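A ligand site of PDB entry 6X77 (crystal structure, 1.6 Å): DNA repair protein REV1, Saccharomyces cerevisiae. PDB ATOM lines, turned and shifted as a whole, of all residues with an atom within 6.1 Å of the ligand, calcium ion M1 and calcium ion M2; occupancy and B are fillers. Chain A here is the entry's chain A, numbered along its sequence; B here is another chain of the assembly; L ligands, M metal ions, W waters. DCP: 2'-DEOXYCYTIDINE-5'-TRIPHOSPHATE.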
ATOM      1  N   ARG A  20      12.107 -22.742 -23.082  1.00  0.00           N
ATOM      2  CA  ARG A  20      12.935 -21.689 -22.489  1.00  0.00           C
ATOM      3  C   ARG A  20      13.011 -21.825 -20.968  1.00  0.00           C
ATOM      4  O   ARG A  20      14.046 -21.458 -20.371  1.00  0.00           O
ATOM      5  CB  ARG A  20      12.428 -20.322 -22.931  1.00  0.00           C
ATOM      6  CG  ARG A  20      11.602 -19.589 -21.904  1.00  0.00           C
ATOM      7  CD  ARG A  20      10.092 -19.939 -21.931  1.00  0.00           C
ATOM      8  NE  ARG A  20       9.336 -19.027 -21.076  1.00  0.00           N
ATOM      9  CZ  ARG A  20       8.032 -19.098 -20.828  1.00  0.00           C
ATOM     10  NH1 ARG A  20       7.269 -20.100 -21.303  1.00  0.00           N
ATOM     11  NH2 ARG A  20       7.481 -18.130 -20.077  1.00  0.00           N
ATOM     12  N   LEU A  21      11.969 -22.360 -20.336  1.00  0.00           N
ATOM     13  CA  LEU A  21      12.035 -22.553 -18.890  1.00  0.00           C
ATOM     14  C   LEU A  21      13.071 -23.620 -18.535  1.00  0.00           C
ATOM     15  O   LEU A  21      13.833 -23.448 -17.574  1.00  0.00           O
ATOM     16  CB  LEU A  21      10.657 -22.884 -18.324  1.00  0.00           C
ATOM     17  CG  LEU A  21       9.653 -21.714 -18.481  1.00  0.00           C
ATOM     18  CD1 LEU A  21       8.298 -22.094 -18.022  1.00  0.00           C
ATOM     19  CD2 LEU A  21      10.083 -20.440 -17.779  1.00  0.00           C
ATOM     20  N   LEU A  24      16.411 -21.746 -18.899  1.00  0.00           N
ATOM     21  CA  LEU A  24      16.640 -20.876 -17.747  1.00  0.00           C
ATOM     22  C   LEU A  24      17.189 -21.657 -16.563  1.00  0.00           C
ATOM     23  O   LEU A  24      18.203 -21.281 -16.000  1.00  0.00           O
ATOM     24  CB  LEU A  24      15.357 -20.169 -17.333  1.00  0.00           C
ATOM     25  CG  LEU A  24      14.977 -19.003 -18.210  1.00  0.00           C
ATOM     26  CD1 LEU A  24      13.659 -18.425 -17.633  1.00  0.00           C
ATOM     27  CD2 LEU A  24      15.991 -17.903 -18.290  1.00  0.00           C
ATOM     28  N   ASP A  58      21.228  -6.322 -14.334  1.00  0.00           N
ATOM     29  CA  ASP A  58      20.281  -7.188 -15.052  1.00  0.00           C
ATOM     30  C   ASP A  58      19.998  -6.654 -16.447  1.00  0.00           C
ATOM     31  O   ASP A  58      19.776  -5.455 -16.632  1.00  0.00           O
ATOM     32  CB  ASP A  58      19.009  -7.303 -14.199  1.00  0.00           C
ATOM     33  CG  ASP A  58      17.848  -7.909 -14.959  1.00  0.00           C
ATOM     34  OD1 ASP A  58      17.743  -9.155 -14.945  1.00  0.00           O
ATOM     35  OD2 ASP A  58      17.110  -7.126 -15.604  1.00  0.00           O
ATOM     36  N   PHE A  59      20.015  -7.557 -17.436  1.00  0.00           N
ATOM     37  CA  PHE A  59      19.699  -7.144 -18.806  1.00  0.00           C
ATOM     38  C   PHE A  59      18.242  -6.671 -18.900  1.00  0.00           C
ATOM     39  O   PHE A  59      17.338  -7.360 -18.416  1.00  0.00           O
ATOM     40  CB  PHE A  59      19.824  -8.313 -19.800  1.00  0.00           C
ATOM     41  CG  PHE A  59      21.205  -8.680 -20.215  1.00  0.00           C
ATOM     42  CD1 PHE A  59      22.000  -9.433 -19.396  1.00  0.00           C
ATOM     43  CD2 PHE A  59      21.617  -8.415 -21.500  1.00  0.00           C
ATOM     44  CE1 PHE A  59      23.264  -9.896 -19.839  1.00  0.00           C
ATOM     45  CE2 PHE A  59      22.851  -8.876 -21.985  1.00  0.00           C
ATOM     46  CZ  PHE A  59      23.679  -9.595 -21.123  1.00  0.00           C
ATOM     47  N   ASP A  60      18.016  -5.530 -19.590  1.00  0.00           N
ATOM     48  CA  ASP A  60      16.665  -5.109 -19.941  1.00  0.00           C
ATOM     49  C   ASP A  60      15.997  -5.950 -21.037  1.00  0.00           C
ATOM     50  O   ASP A  60      16.551  -6.148 -22.129  1.00  0.00           O
ATOM     51  CB  ASP A  60      16.680  -3.668 -20.505  1.00  0.00           C
ATOM     52  CG  ASP A  60      17.314  -2.702 -19.537  1.00  0.00           C
ATOM     53  OD1 ASP A  60      16.954  -2.722 -18.339  1.00  0.00           O
ATOM     54  OD2 ASP A  60      18.194  -1.953 -19.998  1.00  0.00           O
ATOM     55  N   CYS A  61      14.786  -6.439 -20.734  1.00  0.00           N
ATOM     56  CA  CYS A  61      14.008  -7.350 -21.571  1.00  0.00           C
ATOM     57  C   CYS A  61      14.912  -8.295 -22.365  1.00  0.00           C
ATOM     58  O   CYS A  61      14.975  -8.255 -23.602  1.00  0.00           O
ATOM     59  CB  CYS A  61      13.087  -6.577 -22.502  1.00  0.00           C
ATOM     60  SG  CYS A  61      13.887  -5.221 -23.477  1.00  0.00           S
ATOM     61  N   PHE A  62      15.598  -9.173 -21.632  1.00  0.00           N
ATOM     62  CA  PHE A  62      16.757  -9.889 -22.162  1.00  0.00           C
ATOM     63  C   PHE A  62      16.490 -10.623 -23.472  1.00  0.00           C
ATOM     64  O   PHE A  62      17.188 -10.395 -24.458  1.00  0.00           O
ATOM     65  CB  PHE A  62      17.267 -10.848 -21.083  1.00  0.00           C
ATOM     66  CG  PHE A  62      18.460 -11.675 -21.483  1.00  0.00           C
ATOM     67  CD1 PHE A  62      19.623 -11.080 -21.941  1.00  0.00           C
ATOM     68  CD2 PHE A  62      18.432 -13.063 -21.337  1.00  0.00           C
ATOM     69  CE1 PHE A  62      20.720 -11.839 -22.280  1.00  0.00           C
ATOM     70  CE2 PHE A  62      19.558 -13.836 -21.644  1.00  0.00           C
ATOM     71  CZ  PHE A  62      20.683 -13.234 -22.142  1.00  0.00           C
ATOM     72  N   PHE A  63      15.557 -11.584 -23.465  1.00  0.00           N
ATOM     73  CA  PHE A  63      15.361 -12.355 -24.697  1.00  0.00           C
ATOM     74  C   PHE A  63      14.941 -11.422 -25.833  1.00  0.00           C
ATOM     75  O   PHE A  63      15.350 -11.625 -26.968  1.00  0.00           O
ATOM     76  CB  PHE A  63      14.296 -13.450 -24.588  1.00  0.00           C
ATOM     77  CG  PHE A  63      14.707 -14.686 -23.823  1.00  0.00           C
ATOM     78  CD1 PHE A  63      15.910 -14.761 -23.138  1.00  0.00           C
ATOM     79  CD2 PHE A  63      13.862 -15.795 -23.806  1.00  0.00           C
ATOM     80  CE1 PHE A  63      16.239 -15.867 -22.398  1.00  0.00           C
ATOM     81  CE2 PHE A  63      14.194 -16.929 -23.070  1.00  0.00           C
ATOM     82  CZ  PHE A  63      15.383 -16.970 -22.388  1.00  0.00           C
ATOM     83  N   ALA A  64      14.058 -10.453 -25.546  1.00  0.00           N
ATOM     84  CA  ALA A  64      13.587  -9.543 -26.601  1.00  0.00           C
ATOM     85  C   ALA A  64      14.759  -8.767 -27.188  1.00  0.00           C
ATOM     86  O   ALA A  64      14.914  -8.718 -28.416  1.00  0.00           O
ATOM     87  CB  ALA A  64      12.487  -8.620 -26.068  1.00  0.00           C
ATOM     88  N   ASP A  95       3.382 -18.581 -24.616  1.00  0.00           N
ATOM     89  CA  ASP A  95       3.953 -17.626 -23.679  1.00  0.00           C
ATOM     90  C   ASP A  95       4.822 -16.579 -24.382  1.00  0.00           C
ATOM     91  O   ASP A  95       5.663 -16.888 -25.225  1.00  0.00           O
ATOM     92  CB  ASP A  95       4.789 -18.324 -22.616  1.00  0.00           C
ATOM     93  CG  ASP A  95       3.969 -18.926 -21.494  1.00  0.00           C
ATOM     94  OD1 ASP A  95       2.743 -19.148 -21.605  1.00  0.00           O
ATOM     95  OD2 ASP A  95       4.606 -19.240 -20.479  1.00  0.00           O
ATOM     96  N   ILE A  96       4.625 -15.336 -23.986  1.00  0.00           N
ATOM     97  CA  ILE A  96       5.578 -14.261 -24.227  1.00  0.00           C
ATOM     98  C   ILE A  96       6.703 -14.412 -23.198  1.00  0.00           C
ATOM     99  O   ILE A  96       6.575 -14.030 -22.025  1.00  0.00           O
ATOM    100  CB  ILE A  96       4.893 -12.888 -24.145  1.00  0.00           C
ATOM    101  CG1 ILE A  96       3.913 -12.745 -25.323  1.00  0.00           C
ATOM    102  CG2 ILE A  96       5.932 -11.806 -24.160  1.00  0.00           C
ATOM    103  CD1 ILE A  96       2.833 -11.666 -25.075  1.00  0.00           C
ATOM    104  N   ALA A  97       7.838 -14.969 -23.643  1.00  0.00           N
ATOM    105  CA  ALA A  97       8.975 -15.141 -22.738  1.00  0.00           C
ATOM    106  C   ALA A  97       9.535 -13.801 -22.303  1.00  0.00           C
ATOM    107  O   ALA A  97       9.900 -13.649 -21.124  1.00  0.00           O
ATOM    108  CB  ALA A  97      10.077 -16.000 -23.384  1.00  0.00           C
ATOM    109  N   SER A  98       9.614 -12.826 -23.234  1.00  0.00           N
ATOM    110  CA  SER A  98      10.126 -11.476 -22.994  1.00  0.00           C
ATOM    111  C   SER A  98       9.442 -10.521 -23.967  1.00  0.00           C
ATOM    112  O   SER A  98       9.179 -10.892 -25.124  1.00  0.00           O
ATOM    113  CB  SER A  98      11.657 -11.398 -23.133  1.00  0.00           C
ATOM    114  OG  SER A  98      12.212 -10.130 -22.766  1.00  0.00           O
ATOM    115  N   CYS A  99       9.171  -9.309 -23.493  1.00  0.00           N
ATOM    116  CA  CYS A  99       8.621  -8.234 -24.314  1.00  0.00           C
ATOM    117  C   CYS A  99       9.403  -6.963 -24.051  1.00  0.00           C
ATOM    118  O   CYS A  99       9.924  -6.736 -22.934  1.00  0.00           O
ATOM    119  CB  CYS A  99       7.119  -8.044 -24.038  1.00  0.00           C
ATOM    120  SG  CYS A  99       6.711  -7.678 -22.315  1.00  0.00           S
ATOM    121  N   TYR A 101      10.053  -2.675 -24.058  1.00  0.00           N
ATOM    122  CA  TYR A 101       9.337  -1.707 -23.214  1.00  0.00           C
ATOM    123  C   TYR A 101       8.270  -0.975 -23.998  1.00  0.00           C
ATOM    124  O   TYR A 101       7.291  -0.549 -23.385  1.00  0.00           O
ATOM    125  CB  TYR A 101      10.335  -0.760 -22.531  1.00  0.00           C
ATOM    126  CG  TYR A 101      10.931  -1.444 -21.325  1.00  0.00           C
ATOM    127  CD1 TYR A 101      11.817  -2.523 -21.459  1.00  0.00           C
ATOM    128  CD2 TYR A 101      10.569  -1.073 -20.045  1.00  0.00           C
ATOM    129  CE1 TYR A 101      12.302  -3.182 -20.339  1.00  0.00           C
ATOM    130  CE2 TYR A 101      11.063  -1.715 -18.937  1.00  0.00           C
ATOM    131  CZ  TYR A 101      11.929  -2.767 -19.073  1.00  0.00           C
ATOM    132  OH  TYR A 101      12.426  -3.382 -17.944  1.00  0.00           O
ATOM    133  N   ARG A 104       5.392  -3.142 -23.291  1.00  0.00           N
ATOM    134  CA  ARG A 104       4.953  -2.970 -21.912  1.00  0.00           C
ATOM    135  C   ARG A 104       4.192  -1.665 -21.689  1.00  0.00           C
ATOM    136  O   ARG A 104       3.419  -1.570 -20.727  1.00  0.00           O
ATOM    137  CB  ARG A 104       6.150  -3.017 -20.976  1.00  0.00           C
ATOM    138  CG  ARG A 104       6.849  -4.365 -21.009  1.00  0.00           C
ATOM    139  CD  ARG A 104       8.031  -4.432 -20.038  1.00  0.00           C
ATOM    140  NE  ARG A 104       8.857  -5.604 -20.360  1.00  0.00           N
ATOM    141  CZ  ARG A 104       9.792  -6.115 -19.575  1.00  0.00           C
ATOM    142  NH1 ARG A 104      10.050  -5.584 -18.383  1.00  0.00           N
ATOM    143  NH2 ARG A 104      10.460  -7.193 -20.004  1.00  0.00           N
ATOM    144  N   ASN A 110       5.782 -10.065 -19.466  1.00  0.00           N
ATOM    145  CA  ASN A 110       6.354 -11.416 -19.601  1.00  0.00           C
ATOM    146  C   ASN A 110       5.412 -12.440 -18.987  1.00  0.00           C
ATOM    147  O   ASN A 110       4.821 -12.206 -17.922  1.00  0.00           O
ATOM    148  CB  ASN A 110       7.710 -11.511 -18.899  1.00  0.00           C
ATOM    149  CG  ASN A 110       8.797 -10.692 -19.580  1.00  0.00           C
ATOM    150  OD1 ASN A 110       8.595 -10.101 -20.638  1.00  0.00           O
ATOM    151  ND2 ASN A 110       9.969 -10.643 -18.949  1.00  0.00           N
ATOM    152  N   GLY A 111       5.246 -13.563 -19.668  1.00  0.00           N
ATOM    153  CA  GLY A 111       4.380 -14.638 -19.225  1.00  0.00           C
ATOM    154  C   GLY A 111       2.976 -14.593 -19.785  1.00  0.00           C
ATOM    155  O   GLY A 111       2.271 -15.611 -19.738  1.00  0.00           O
ATOM    156  N   TYR A 132      12.918 -17.535 -30.576  1.00  0.00           N
ATOM    157  CA  TYR A 132      13.997 -17.696 -29.638  1.00  0.00           C
ATOM    158  C   TYR A 132      15.334 -17.853 -30.363  1.00  0.00           C
ATOM    159  O   TYR A 132      15.418 -18.491 -31.411  1.00  0.00           O
ATOM    160  CB  TYR A 132      13.750 -18.925 -28.781  1.00  0.00           C
ATOM    161  CG  TYR A 132      12.525 -18.862 -27.869  1.00  0.00           C
ATOM    162  CD1 TYR A 132      11.282 -19.317 -28.278  1.00  0.00           C
ATOM    163  CD2 TYR A 132      12.632 -18.365 -26.581  1.00  0.00           C
ATOM    164  CE1 TYR A 132      10.191 -19.311 -27.419  1.00  0.00           C
ATOM    165  CE2 TYR A 132      11.517 -18.296 -25.741  1.00  0.00           C
ATOM    166  CZ  TYR A 132      10.319 -18.796 -26.149  1.00  0.00           C
ATOM    167  OH  TYR A 132       9.225 -18.817 -25.311  1.00  0.00           O
ATOM    168  N   SER A 161      20.839 -15.333 -12.528  1.00  0.00           N
ATOM    169  CA  SER A 161      20.303 -16.044 -13.685  1.00  0.00           C
ATOM    170  C   SER A 161      21.167 -15.678 -14.893  1.00  0.00           C
ATOM    171  O   SER A 161      22.173 -14.973 -14.785  1.00  0.00           O
ATOM    172  CB  SER A 161      18.834 -15.701 -13.912  1.00  0.00           C
ATOM    173  OG  SER A 161      18.764 -14.398 -14.477  1.00  0.00           O
ATOM    174  N   ILE A 162      20.783 -16.245 -16.031  1.00  0.00           N
ATOM    175  CA  ILE A 162      21.426 -16.033 -17.308  1.00  0.00           C
ATOM    176  C   ILE A 162      21.703 -14.538 -17.517  1.00  0.00           C
ATOM    177  O   ILE A 162      22.755 -14.177 -18.047  1.00  0.00           O
ATOM    178  CB  ILE A 162      20.539 -16.609 -18.434  1.00  0.00           C
ATOM    179  CG1 ILE A 162      21.309 -16.562 -19.769  1.00  0.00           C
ATOM    180  CG2 ILE A 162      19.154 -15.972 -18.510  1.00  0.00           C
ATOM    181  CD1 ILE A 162      22.416 -17.492 -19.793  1.00  0.00           C
ATOM    182  N   ASP A 163      20.790 -13.659 -17.098  1.00  0.00           N
ATOM    183  CA  ASP A 163      20.934 -12.238 -17.413  1.00  0.00           C
ATOM    184  C   ASP A 163      21.079 -11.344 -16.185  1.00  0.00           C
ATOM    185  O   ASP A 163      20.848 -10.125 -16.302  1.00  0.00           O
ATOM    186  CB  ASP A 163      19.742 -11.765 -18.255  1.00  0.00           C
ATOM    187  CG  ASP A 163      18.499 -11.461 -17.394  1.00  0.00           C
ATOM    188  OD1 ASP A 163      18.299 -12.172 -16.389  1.00  0.00           O
ATOM    189  OD2 ASP A 163      17.745 -10.539 -17.767  1.00  0.00           O
ATOM    190  N   GLU A 164      21.507 -11.882 -15.046  1.00  0.00           N
ATOM    191  CA  GLU A 164      21.359 -11.123 -13.806  1.00  0.00           C
ATOM    192  C   GLU A 164      22.361 -11.570 -12.764  1.00  0.00           C
ATOM    193  O   GLU A 164      22.537 -12.779 -12.541  1.00  0.00           O
ATOM    194  CB  GLU A 164      19.942 -11.283 -13.277  1.00  0.00           C
ATOM    195  CG  GLU A 164      19.583 -10.502 -12.065  1.00  0.00           C
ATOM    196  CD  GLU A 164      18.112 -10.664 -11.687  1.00  0.00           C
ATOM    197  OE1 GLU A 164      17.747 -10.174 -10.579  1.00  0.00           O
ATOM    198  OE2 GLU A 164      17.340 -11.331 -12.466  1.00  0.00           O
ATOM    199  N   LYS A 218      14.508  -2.052 -10.265  1.00  0.00           N
ATOM    200  CA  LYS A 218      13.185  -1.845 -10.843  1.00  0.00           C
ATOM    201  C   LYS A 218      12.963  -0.382 -11.212  1.00  0.00           C
ATOM    202  O   LYS A 218      12.523  -0.064 -12.310  1.00  0.00           O
ATOM    203  CB  LYS A 218      12.131  -2.302  -9.849  1.00  0.00           C
ATOM    204  CG  LYS A 218      10.751  -2.416 -10.430  1.00  0.00           C
ATOM    205  CD  LYS A 218      10.725  -3.644 -11.255  1.00  0.00           C
ATOM    206  CE  LYS A 218       9.962  -3.428 -12.540  1.00  0.00           C
ATOM    207  NZ  LYS A 218       8.857  -2.399 -12.446  1.00  0.00           N
ATOM    208  N   LYS A 221      14.898   0.845 -14.492  1.00  0.00           N
ATOM    209  CA  LYS A 221      14.567   0.341 -15.816  1.00  0.00           C
ATOM    210  C   LYS A 221      13.608   1.262 -16.573  1.00  0.00           C
ATOM    211  O   LYS A 221      12.767   1.926 -15.961  1.00  0.00           O
ATOM    212  CB  LYS A 221      13.958  -1.041 -15.680  1.00  0.00           C
ATOM    213  CG  LYS A 221      15.003  -2.128 -15.330  1.00  0.00           C
ATOM    214  CD  LYS A 221      14.410  -3.500 -15.146  1.00  0.00           C
ATOM    215  CE  LYS A 221      15.542  -4.530 -15.015  1.00  0.00           C
ATOM    216  NZ  LYS A 221      16.186  -4.791 -16.348  1.00  0.00           N
ATOM    217  P    DG B  12      15.239 -14.557  -8.906  1.00  0.00           P
ATOM    218  OP1  DG B  12      16.075 -15.282  -8.046  1.00  0.00           O
ATOM    219  OP2  DG B  12      14.925 -13.200  -8.619  1.00  0.00           O
ATOM    220  O5'  DG B  12      15.913 -14.696 -10.336  1.00  0.00           O
ATOM    221  C5'  DG B  12      15.478 -13.920 -11.435  1.00  0.00           C
ATOM    222  C4'  DG B  12      15.225 -14.807 -12.643  1.00  0.00           C
ATOM    223  O4'  DG B  12      14.099 -15.609 -12.405  1.00  0.00           O
ATOM    224  C3'  DG B  12      14.872 -14.019 -13.888  1.00  0.00           C
ATOM    225  O3'  DG B  12      16.036 -13.729 -14.625  1.00  0.00           O
ATOM    226  C2'  DG B  12      13.932 -14.945 -14.634  1.00  0.00           C
ATOM    227  C1'  DG B  12      13.694 -16.085 -13.668  1.00  0.00           C
ATOM    228  N9   DG B  12      12.334 -16.569 -13.567  1.00  0.00           N
ATOM    229  C8   DG B  12      11.159 -15.868 -13.492  1.00  0.00           C
ATOM    230  N7   DG B  12      10.115 -16.643 -13.400  1.00  0.00           N
ATOM    231  C5   DG B  12      10.632 -17.925 -13.446  1.00  0.00           C
ATOM    232  C6   DG B  12       9.972 -19.184 -13.379  1.00  0.00           C
ATOM    233  O6   DG B  12       8.784 -19.418 -13.345  1.00  0.00           O
ATOM    234  N1   DG B  12      10.884 -20.231 -13.447  1.00  0.00           N
ATOM    235  C2   DG B  12      12.241 -20.093 -13.539  1.00  0.00           C
ATOM    236  N2   DG B  12      12.935 -21.226 -13.639  1.00  0.00           N
ATOM    237  N3   DG B  12      12.862 -18.932 -13.609  1.00  0.00           N
ATOM    238  C4   DG B  12      11.998 -17.898 -13.560  1.00  0.00           C
HETATM  239  N1  DCP L   1      11.689 -15.340 -18.794  1.00  0.00           N
HETATM  240  C2  DCP L   1      10.650 -16.198 -19.424  1.00  0.00           C
HETATM  241  N3  DCP L   1       9.305 -16.198 -18.835  1.00  0.00           N
HETATM  242  C4  DCP L   1       8.989 -15.325 -17.761  1.00  0.00           C
HETATM  243  C5  DCP L   1      10.011 -14.437 -17.164  1.00  0.00           C
HETATM  244  C6  DCP L   1      11.381 -14.446 -17.710  1.00  0.00           C
HETATM  245  O2  DCP L   1      10.845 -16.925 -20.327  1.00  0.00           O
HETATM  246  N4  DCP L   1       7.669 -15.284 -17.253  1.00  0.00           N
HETATM  247  C1' DCP L   1      13.053 -15.298 -19.354  1.00  0.00           C
HETATM  248  C2' DCP L   1      12.936 -14.254 -20.529  1.00  0.00           C
HETATM  249  C3' DCP L   1      13.463 -12.981 -19.916  1.00  0.00           C
HETATM  250  C4' DCP L   1      14.499 -13.461 -19.177  1.00  0.00           C
HETATM  251  O4' DCP L   1      13.917 -14.813 -18.526  1.00  0.00           O
HETATM  252  O3' DCP L   1      14.120 -12.125 -20.917  1.00  0.00           O
HETATM  253  C5' DCP L   1      15.023 -12.771 -17.975  1.00  0.00           C
HETATM  254  O5' DCP L   1      13.943 -12.626 -17.067  1.00  0.00           O
HETATM  255  PA  DCP L   1      13.704 -11.193 -16.365  1.00  0.00           P
HETATM  256  O1A DCP L   1      14.978 -10.603 -15.850  1.00  0.00           O
HETATM  257  O2A DCP L   1      12.645 -11.381 -15.286  1.00  0.00           O
HETATM  258  O3A DCP L   1      12.953 -10.275 -17.455  1.00  0.00           O
HETATM  259  PB  DCP L   1      13.367  -9.468 -18.776  1.00  0.00           P
HETATM  260  O1B DCP L   1      14.868  -9.394 -18.851  1.00  0.00           O
HETATM  261  O2B DCP L   1      12.685 -10.015 -20.017  1.00  0.00           O
HETATM  262  O3B DCP L   1      12.763  -8.016 -18.494  1.00  0.00           O
HETATM  263  PG  DCP L   1      13.201  -6.922 -17.338  1.00  0.00           P
HETATM  264  O1G DCP L   1      14.259  -7.516 -16.455  1.00  0.00           O
HETATM  265  O2G DCP L   1      13.753  -5.724 -18.053  1.00  0.00           O
HETATM  266  O3G DCP L   1      11.910  -6.609 -16.608  1.00  0.00           O
HETATM  267 CA    CA M   1      16.712 -11.413 -14.782  1.00  0.00          CA
HETATM  268 CA    CA M   2      16.224  -8.899 -17.039  1.00  0.00          CA
HETATM  269  O   HOH W   1      14.153  -7.815 -13.556  1.00  0.00           O
HETATM  270  O   HOH W   2      11.998 -12.432 -12.679  1.00  0.00           O
HETATM  271  O   HOH W   3       7.099 -13.833 -14.848  1.00  0.00           O
HETATM  272  O   HOH W   4      11.566  -5.437 -14.157  1.00  0.00           O
HETATM  273  O   HOH W   5       9.930 -11.205 -16.125  1.00  0.00           O
HETATM  274  O   HOH W   6       9.968  -8.367 -16.161  1.00  0.00           O
HETATM  275  O   HOH W   7       5.707 -17.474 -17.565  1.00  0.00           O
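An oxygen (O2B) of the ligand sits at hydrogen-bond distance from the side-chain hydroxyl (OG) of Ser 98 (2.8 Å).
An oxygen (O3') of the ligand sits at hydrogen-bond distance from the backbone NH (N) of Phe 62, 3.4 Å away.
An oxygen (O2B) of the ligand lies within hydrogen-bond range of the side-chain amide nitrogen (ND2) of Asn 110 (3.0 Å).
The side-chain hydroxyl (OH) of Tyr 101 is in hydrogen-bond range of an oxygen (O2G) of the ligand, 2.7 Å away.
The side-chain amino group of Lys 221 lies within salt-bridge range of an oxygen (O2G) of the ligand, 3.1 Å away.
The backbone NH (N) of Cys 61 is in hydrogen-bond range of an oxygen (O2G) of the ligand (3.0 Å).
N of Phe 63 lies within hydrogen-bond range of O3' of the ligand.
The guanidinium group (NE) of Arg 20 lies within hydrogen-bond range of an oxygen (O2) of the ligand, at 2.7 Å.
NH1 of Arg 104 lies within salt-bridge range of O3G of the ligand, at 2.8 Å.
The side-chain amino group (NZ) of Lys 221 is in salt-bridge range of the side-chain carboxylate (OD1) of Asp 60 (3.0 Å).
NE of Arg 104 is in hydrogen-bond range of O of Cys 99, at 3.0 Å.
The backbone NH (N) of Asp 163 sits close to the side-chain hydroxyl (OG) of Ser 161, at 3.4 Å.
NH1 of Arg 20 lies within salt-bridge range of OD2 of Asp 95, 2.9 Å away.
O of Ile 96 is in hydrogen-bond range of N of Gly 111 (2.7 Å).
N of Cys 99 sits at hydrogen-bond distance from OD1 of Asn 110 (3.0 Å).
The backbone NH (N) of Ala 64 is in hydrogen-bond range of the side-chain hydroxyl (OG) of Ser 98 (3.4 Å).
OG of Ser 98 lies close to O of Cys 61, 3.4 Å away.
O of Ala 97 sits close to N1 of the ligand.
Leu 24 touches the ligand (CD1 to C1', 3.6 Å).
Asp 60 touches the ligand.
Gly 111 touches the ligand.
17 residues have an atom within 4 Å of the ligand: Arg 20, Leu 24, Asp 58, Phe 59, Asp 60, Cys 61, Phe 62, Phe 63, Ala 97, Ser 98, Tyr 101, Arg 104, Asn 110, Gly 111, Asp 163, Lys 221 and DG 12 of chain B.
The nearest printed residue that does not touch the ligand is Glu 164 (4.2 Å).
Residues that only touch calcium ion M1: Ser 161.
Of the 27 residues printed, 5 come within 4 Å of calcium ion M1.
Along chain A the residues within 4 Å of calcium ion M1 span positions 58 to 164.
The nearest printed residue that does not touch calcium ion M1 is Phe 59 (5.5 Å).
Within 4 Å of calcium ion M2: Asp 58, Phe 59 and Asp 163.
Calcium ion M1 is bound by an oxygen (O1A) of the ligand, the side-chain carboxylate of Asp 163, the side-chain carboxylate of Glu 164, O3' of DG 12 of chain B and the side-chain carboxylate of Asp 58.
Calcium ion M1 has five donor atoms within binding distance.
Calcium ion M2 is bound by an oxygen (O1B) of the ligand, the backbone carbonyl oxygen (O) of Phe 59, the side-chain carboxylate (OD2) of Asp 163, an oxygen (O1A) of the ligand, the side-chain carboxylate (OD2) of Asp 58, an oxygen (O1G) of the ligand and the side-chain carboxylate (OD1) of Asp 58.
Water W5 bridges O2A of the ligand and ND2 of Asn 110.
Water W7 lies within hydrogen-bond range of N4 of the ligand (3.0 Å) and NH2 of Arg 20 (3.1 Å).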
